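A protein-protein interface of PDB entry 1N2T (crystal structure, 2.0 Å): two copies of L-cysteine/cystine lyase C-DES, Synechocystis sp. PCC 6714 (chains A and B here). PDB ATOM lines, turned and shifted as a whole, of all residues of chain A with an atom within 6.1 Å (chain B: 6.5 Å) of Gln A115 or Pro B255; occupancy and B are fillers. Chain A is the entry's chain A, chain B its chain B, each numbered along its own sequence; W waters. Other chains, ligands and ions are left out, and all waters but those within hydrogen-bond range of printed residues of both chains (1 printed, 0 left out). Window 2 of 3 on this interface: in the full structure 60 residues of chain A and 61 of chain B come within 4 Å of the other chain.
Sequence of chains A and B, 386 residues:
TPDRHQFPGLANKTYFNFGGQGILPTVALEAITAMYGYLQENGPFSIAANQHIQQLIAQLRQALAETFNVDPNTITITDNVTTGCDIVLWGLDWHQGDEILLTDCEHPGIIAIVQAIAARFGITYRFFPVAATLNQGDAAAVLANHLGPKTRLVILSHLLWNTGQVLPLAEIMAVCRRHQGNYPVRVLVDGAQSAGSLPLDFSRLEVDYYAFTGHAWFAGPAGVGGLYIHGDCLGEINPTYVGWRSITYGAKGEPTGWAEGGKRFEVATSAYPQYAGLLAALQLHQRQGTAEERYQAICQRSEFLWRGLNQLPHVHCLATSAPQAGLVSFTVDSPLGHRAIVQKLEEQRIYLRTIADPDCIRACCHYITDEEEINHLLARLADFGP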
ATOM      1  N   PRO A 108      21.249 -26.639  -6.344  1.00  0.00           N
ATOM      2  CA  PRO A 108      22.473 -26.532  -7.152  1.00  0.00           C
ATOM      3  C   PRO A 108      22.925 -27.894  -7.703  1.00  0.00           C
ATOM      4  O   PRO A 108      23.342 -27.999  -8.850  1.00  0.00           O
ATOM      5  CB  PRO A 108      23.489 -25.973  -6.163  1.00  0.00           C
ATOM      6  CG  PRO A 108      22.632 -25.122  -5.266  1.00  0.00           C
ATOM      7  CD  PRO A 108      21.429 -25.998  -5.027  1.00  0.00           C
ATOM      8  N   GLY A 109      22.849 -28.922  -6.864  1.00  0.00           N
ATOM      9  CA  GLY A 109      23.242 -30.259  -7.282  1.00  0.00           C
ATOM     10  C   GLY A 109      22.434 -30.782  -8.459  1.00  0.00           C
ATOM     11  O   GLY A 109      22.991 -31.458  -9.325  1.00  0.00           O
ATOM     12  N   ILE A 110      21.130 -30.482  -8.475  1.00  0.00           N
ATOM     13  CA  ILE A 110      20.227 -30.906  -9.548  1.00  0.00           C
ATOM     14  C   ILE A 110      20.582 -30.153 -10.843  1.00  0.00           C
ATOM     15  O   ILE A 110      20.667 -30.737 -11.925  1.00  0.00           O
ATOM     16  CB  ILE A 110      18.757 -30.620  -9.152  1.00  0.00           C
ATOM     17  CG1 ILE A 110      18.429 -31.325  -7.836  1.00  0.00           C
ATOM     18  CG2 ILE A 110      17.814 -31.034 -10.254  1.00  0.00           C
ATOM     19  CD1 ILE A 110      18.993 -32.725  -7.681  1.00  0.00           C
ATOM     20  N   ILE A 111      20.788 -28.849 -10.729  1.00  0.00           N
ATOM     21  CA  ILE A 111      21.191 -28.049 -11.879  1.00  0.00           C
ATOM     22  C   ILE A 111      22.491 -28.665 -12.491  1.00  0.00           C
ATOM     23  O   ILE A 111      22.652 -28.738 -13.715  1.00  0.00           O
ATOM     24  CB  ILE A 111      21.436 -26.570 -11.426  1.00  0.00           C
ATOM     25  CG1 ILE A 111      20.128 -25.959 -10.916  1.00  0.00           C
ATOM     26  CG2 ILE A 111      22.008 -25.745 -12.582  1.00  0.00           C
ATOM     27  CD1 ILE A 111      20.263 -24.529 -10.291  1.00  0.00           C
ATOM     28  N   ALA A 112      23.403 -29.143 -11.643  1.00  0.00           N
ATOM     29  CA  ALA A 112      24.658 -29.729 -12.149  1.00  0.00           C
ATOM     30  C   ALA A 112      24.434 -30.951 -13.047  1.00  0.00           C
ATOM     31  O   ALA A 112      25.120 -31.129 -14.057  1.00  0.00           O
ATOM     32  CB  ALA A 112      25.585 -30.104 -10.983  1.00  0.00           C
ATOM     33  N   ILE A 113      23.481 -31.801 -12.687  1.00  0.00           N
ATOM     34  CA  ILE A 113      23.184 -32.970 -13.507  1.00  0.00           C
ATOM     35  C   ILE A 113      22.698 -32.482 -14.881  1.00  0.00           C
ATOM     36  O   ILE A 113      23.149 -32.965 -15.923  1.00  0.00           O
ATOM     37  CB  ILE A 113      22.048 -33.826 -12.883  1.00  0.00           C
ATOM     38  CG1 ILE A 113      22.415 -34.240 -11.461  1.00  0.00           C
ATOM     39  CG2 ILE A 113      21.795 -35.072 -13.744  1.00  0.00           C
ATOM     40  CD1 ILE A 113      21.266 -34.924 -10.719  1.00  0.00           C
ATOM     41  N   VAL A 114      21.757 -31.541 -14.869  1.00  0.00           N
ATOM     42  CA  VAL A 114      21.196 -30.977 -16.094  1.00  0.00           C
ATOM     43  C   VAL A 114      22.276 -30.397 -17.002  1.00  0.00           C
ATOM     44  O   VAL A 114      22.218 -30.569 -18.219  1.00  0.00           O
ATOM     45  CB  VAL A 114      20.143 -29.871 -15.775  1.00  0.00           C
ATOM     46  CG1 VAL A 114      19.741 -29.134 -17.055  1.00  0.00           C
ATOM     47  CG2 VAL A 114      18.884 -30.516 -15.134  1.00  0.00           C
ATOM     48  N   GLN A 115      23.264 -29.728 -16.418  1.00  0.00           N
ATOM     49  CA  GLN A 115      24.338 -29.131 -17.212  1.00  0.00           C
ATOM     50  C   GLN A 115      25.180 -30.255 -17.806  1.00  0.00           C
ATOM     51  O   GLN A 115      25.640 -30.182 -18.952  1.00  0.00           O
ATOM     52  CB  GLN A 115      25.193 -28.196 -16.330  1.00  0.00           C
ATOM     53  CG  GLN A 115      24.378 -27.031 -15.751  1.00  0.00           C
ATOM     54  CD  GLN A 115      25.196 -26.121 -14.852  1.00  0.00           C
ATOM     55  OE1 GLN A 115      25.980 -26.587 -14.036  1.00  0.00           O
ATOM     56  NE2 GLN A 115      25.003 -24.822 -14.991  1.00  0.00           N
ATOM     57  N   ALA A 116      25.372 -31.305 -17.020  1.00  0.00           N
ATOM     58  CA  ALA A 116      26.134 -32.458 -17.469  1.00  0.00           C
ATOM     59  C   ALA A 116      25.385 -33.129 -18.633  1.00  0.00           C
ATOM     60  O   ALA A 116      25.985 -33.575 -19.605  1.00  0.00           O
ATOM     61  CB  ALA A 116      26.299 -33.443 -16.316  1.00  0.00           C
ATOM     62  N   ILE A 117      24.063 -33.199 -18.520  1.00  0.00           N
ATOM     63  CA  ILE A 117      23.233 -33.802 -19.560  1.00  0.00           C
ATOM     64  C   ILE A 117      23.259 -32.954 -20.826  1.00  0.00           C
ATOM     65  O   ILE A 117      23.264 -33.491 -21.939  1.00  0.00           O
ATOM     66  CB  ILE A 117      21.741 -33.910 -19.125  1.00  0.00           C
ATOM     67  CG1 ILE A 117      21.600 -34.818 -17.908  1.00  0.00           C
ATOM     68  CG2 ILE A 117      20.914 -34.453 -20.258  1.00  0.00           C
ATOM     69  CD1 ILE A 117      22.060 -36.246 -18.160  1.00  0.00           C
ATOM     70  N   ALA A 118      23.234 -31.635 -20.656  1.00  0.00           N
ATOM     71  CA  ALA A 118      23.241 -30.729 -21.802  1.00  0.00           C
ATOM     72  C   ALA A 118      24.524 -30.922 -22.581  1.00  0.00           C
ATOM     73  O   ALA A 118      24.510 -30.971 -23.805  1.00  0.00           O
ATOM     74  CB  ALA A 118      23.125 -29.250 -21.334  1.00  0.00           C
ATOM     75  N   ALA A 119      25.637 -31.029 -21.864  1.00  0.00           N
ATOM     76  CA  ALA A 119      26.932 -31.184 -22.508  1.00  0.00           C
ATOM     77  C   ALA A 119      27.050 -32.522 -23.231  1.00  0.00           C
ATOM     78  O   ALA A 119      27.616 -32.607 -24.320  1.00  0.00           O
ATOM     79  CB  ALA A 119      28.040 -31.056 -21.481  1.00  0.00           C
ATOM     80  N   ARG A 120      26.499 -33.569 -22.630  1.00  0.00           N
ATOM     81  CA  ARG A 120      26.594 -34.902 -23.207  1.00  0.00           C
ATOM     82  C   ARG A 120      25.675 -35.196 -24.395  1.00  0.00           C
ATOM     83  O   ARG A 120      26.114 -35.779 -25.386  1.00  0.00           O
ATOM     84  CB  ARG A 120      26.332 -35.947 -22.131  1.00  0.00           C
ATOM     85  CG  ARG A 120      26.851 -37.314 -22.490  1.00  0.00           C
ATOM     86  CD  ARG A 120      28.356 -37.358 -22.253  1.00  0.00           C
ATOM     87  NE  ARG A 120      28.674 -37.218 -20.830  1.00  0.00           N
ATOM     88  CZ  ARG A 120      28.876 -38.248 -20.009  1.00  0.00           C
ATOM     89  NH1 ARG A 120      28.799 -39.491 -20.478  1.00  0.00           N
ATOM     90  NH2 ARG A 120      29.139 -38.044 -18.721  1.00  0.00           N
ATOM     91  N   TYR A 125      18.475 -26.071 -21.719  1.00  0.00           N
ATOM     92  CA  TYR A 125      17.667 -25.895 -20.515  1.00  0.00           C
ATOM     93  C   TYR A 125      17.434 -24.415 -20.217  1.00  0.00           C
ATOM     94  O   TYR A 125      18.282 -23.576 -20.514  1.00  0.00           O
ATOM     95  CB  TYR A 125      18.318 -26.595 -19.306  1.00  0.00           C
ATOM     96  CG  TYR A 125      19.596 -25.960 -18.827  1.00  0.00           C
ATOM     97  CD1 TYR A 125      19.576 -24.985 -17.839  1.00  0.00           C
ATOM     98  CD2 TYR A 125      20.828 -26.319 -19.375  1.00  0.00           C
ATOM     99  CE1 TYR A 125      20.744 -24.378 -17.400  1.00  0.00           C
ATOM    100  CE2 TYR A 125      22.013 -25.715 -18.945  1.00  0.00           C
ATOM    101  CZ  TYR A 125      21.956 -24.748 -17.953  1.00  0.00           C
ATOM    102  OH  TYR A 125      23.110 -24.163 -17.494  1.00  0.00           O
ATOM    103  N   ILE B 247      30.585 -30.355  -7.180  1.00  0.00           N
ATOM    104  CA  ILE B 247      30.904 -29.020  -7.684  1.00  0.00           C
ATOM    105  C   ILE B 247      31.494 -27.986  -6.735  1.00  0.00           C
ATOM    106  O   ILE B 247      31.557 -28.201  -5.532  1.00  0.00           O
ATOM    107  CB  ILE B 247      29.613 -28.409  -8.241  1.00  0.00           C
ATOM    108  CG1 ILE B 247      28.593 -28.285  -7.098  1.00  0.00           C
ATOM    109  CG2 ILE B 247      29.054 -29.302  -9.331  1.00  0.00           C
ATOM    110  CD1 ILE B 247      27.231 -27.658  -7.485  1.00  0.00           C
ATOM    111  N   THR B 248      31.900 -26.852  -7.311  1.00  0.00           N
ATOM    112  CA  THR B 248      32.409 -25.704  -6.550  1.00  0.00           C
ATOM    113  C   THR B 248      31.249 -24.719  -6.656  1.00  0.00           C
ATOM    114  O   THR B 248      30.434 -24.807  -7.583  1.00  0.00           O
ATOM    115  CB  THR B 248      33.693 -25.072  -7.179  1.00  0.00           C
ATOM    116  OG1 THR B 248      33.502 -24.862  -8.583  1.00  0.00           O
ATOM    117  CG2 THR B 248      34.902 -25.976  -6.933  1.00  0.00           C
ATOM    118  N   TYR B 249      31.168 -23.786  -5.717  1.00  0.00           N
ATOM    119  CA  TYR B 249      30.063 -22.845  -5.689  1.00  0.00           C
ATOM    120  C   TYR B 249      30.409 -21.379  -5.917  1.00  0.00           C
ATOM    121  O   TYR B 249      31.488 -20.915  -5.537  1.00  0.00           O
ATOM    122  CB  TYR B 249      29.344 -22.983  -4.352  1.00  0.00           C
ATOM    123  CG  TYR B 249      28.702 -24.336  -4.169  1.00  0.00           C
ATOM    124  CD1 TYR B 249      29.445 -25.446  -3.749  1.00  0.00           C
ATOM    125  CD2 TYR B 249      27.352 -24.517  -4.453  1.00  0.00           C
ATOM    126  CE1 TYR B 249      28.846 -26.713  -3.616  1.00  0.00           C
ATOM    127  CE2 TYR B 249      26.750 -25.765  -4.326  1.00  0.00           C
ATOM    128  CZ  TYR B 249      27.491 -26.850  -3.911  1.00  0.00           C
ATOM    129  OH  TYR B 249      26.854 -28.062  -3.789  1.00  0.00           O
ATOM    130  N   GLY B 250      29.466 -20.659  -6.519  1.00  0.00           N
ATOM    131  CA  GLY B 250      29.655 -19.249  -6.799  1.00  0.00           C
ATOM    132  C   GLY B 250      29.048 -18.350  -5.734  1.00  0.00           C
ATOM    133  O   GLY B 250      28.519 -18.830  -4.725  1.00  0.00           O
ATOM    134  N   GLY B 253      25.629 -19.105  -4.582  1.00  0.00           N
ATOM    135  CA  GLY B 253      25.454 -20.535  -4.375  1.00  0.00           C
ATOM    136  C   GLY B 253      25.190 -21.357  -5.625  1.00  0.00           C
ATOM    137  O   GLY B 253      24.711 -22.489  -5.543  1.00  0.00           O
ATOM    138  N   GLU B 254      25.500 -20.789  -6.784  1.00  0.00           N
ATOM    139  CA  GLU B 254      25.304 -21.470  -8.059  1.00  0.00           C
ATOM    140  C   GLU B 254      26.545 -22.287  -8.462  1.00  0.00           C
ATOM    141  O   GLU B 254      27.653 -21.986  -8.026  1.00  0.00           O
ATOM    142  CB  GLU B 254      24.980 -20.441  -9.143  1.00  0.00           C
ATOM    143  CG  GLU B 254      26.177 -19.638  -9.681  1.00  0.00           C
ATOM    144  CD  GLU B 254      26.727 -18.598  -8.709  1.00  0.00           C
ATOM    145  OE1 GLU B 254      27.689 -17.895  -9.083  1.00  0.00           O
ATOM    146  OE2 GLU B 254      26.212 -18.471  -7.580  1.00  0.00           O
ATOM    147  N   PRO B 255      26.367 -23.339  -9.286  1.00  0.00           N
ATOM    148  CA  PRO B 255      27.486 -24.183  -9.732  1.00  0.00           C
ATOM    149  C   PRO B 255      28.494 -23.403 -10.582  1.00  0.00           C
ATOM    150  O   PRO B 255      28.113 -22.742 -11.548  1.00  0.00           O
ATOM    151  CB  PRO B 255      26.794 -25.278 -10.547  1.00  0.00           C
ATOM    152  CG  PRO B 255      25.429 -25.365  -9.932  1.00  0.00           C
ATOM    153  CD  PRO B 255      25.083 -23.912  -9.727  1.00  0.00           C
ATOM    154  N   THR B 256      29.774 -23.466 -10.228  1.00  0.00           N
ATOM    155  CA  THR B 256      30.781 -22.760 -11.011  1.00  0.00           C
ATOM    156  C   THR B 256      31.830 -23.670 -11.650  1.00  0.00           C
ATOM    157  O   THR B 256      32.664 -23.201 -12.422  1.00  0.00           O
ATOM    158  CB  THR B 256      31.510 -21.707 -10.170  1.00  0.00           C
ATOM    159  OG1 THR B 256      32.114 -22.321  -9.024  1.00  0.00           O
ATOM    160  CG2 THR B 256      30.538 -20.634  -9.725  1.00  0.00           C
ATOM    161  N   GLY B 257      31.782 -24.963 -11.340  1.00  0.00           N
ATOM    162  CA  GLY B 257      32.742 -25.893 -11.905  1.00  0.00           C
ATOM    163  C   GLY B 257      32.833 -27.178 -11.095  1.00  0.00           C
ATOM    164  O   GLY B 257      32.078 -27.364 -10.126  1.00  0.00           O
HETATM  165  O   HOH W   1      27.488 -22.749 -14.653  1.00  0.00           O
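NE2 of Gln A115 is in hydrogen-bond range of OH of Tyr A125, 3.2 Å away.
CB of Pro A108 touches CE2 of Tyr B249, 3.7 Å away.
Pro A108 touches Gly B253.
Pro B255 touches Pro A108 (CG to O, 3.5 Å).
CG2 of Ile B247 touches CB of Ala A112, at 3.9 Å.
Gln A115 touches Pro B255 (OE1 to CB, 3.8 Å).
Of chain B, only Pro B255 comes within 4 Å of Gln A115.
Pro B255 touches two residues of chain A.
Of the printed residues of chain A, Tyr B249 touches Pro A108.
Of the printed residues of chain A, Gly B253 touches Pro A108 (3.4 Å).
Of the printed residues of chain A, Ile B247 touches Ala A112.
Of the printed residues of chain B, Ala A112 touches Ile B247.
Of the printed residues of chain B, Pro A108 touches Tyr B249 (3.7 Å), Gly B253 (3.4 Å) and Pro B255 (3.5 Å).
The nearest printed residue of chain B that does not touch Gln A115 is Thr B256 (6.2 Å).
The nearest residue of chain A that does not touch Pro B255 is Ile A111 (4.3 Å).
Printed residues of chain B that touch a printed residue of chain A: Ile B247, Tyr B249, Gly B253 and Pro B255.
Hydrophobic or aromatic side chains of chain B that line the printed part of chain A: Ile B247, Tyr B249 and Pro B255.
Hydrophobic or aromatic side chains of chain A that line the printed part of chain B: Pro A108 and Ala A112.
Among the printed residues, no Asp or Glu carboxylate lies within 4 Å of a Lys or Arg side-chain nitrogen of the other chain.
No position is printed for both chains.
Water W1 bridges the backbone carbonyl oxygen of Pro B255 (3.2 Å) and the side-chain amide nitrogen of Gln A115 (3.3 Å).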
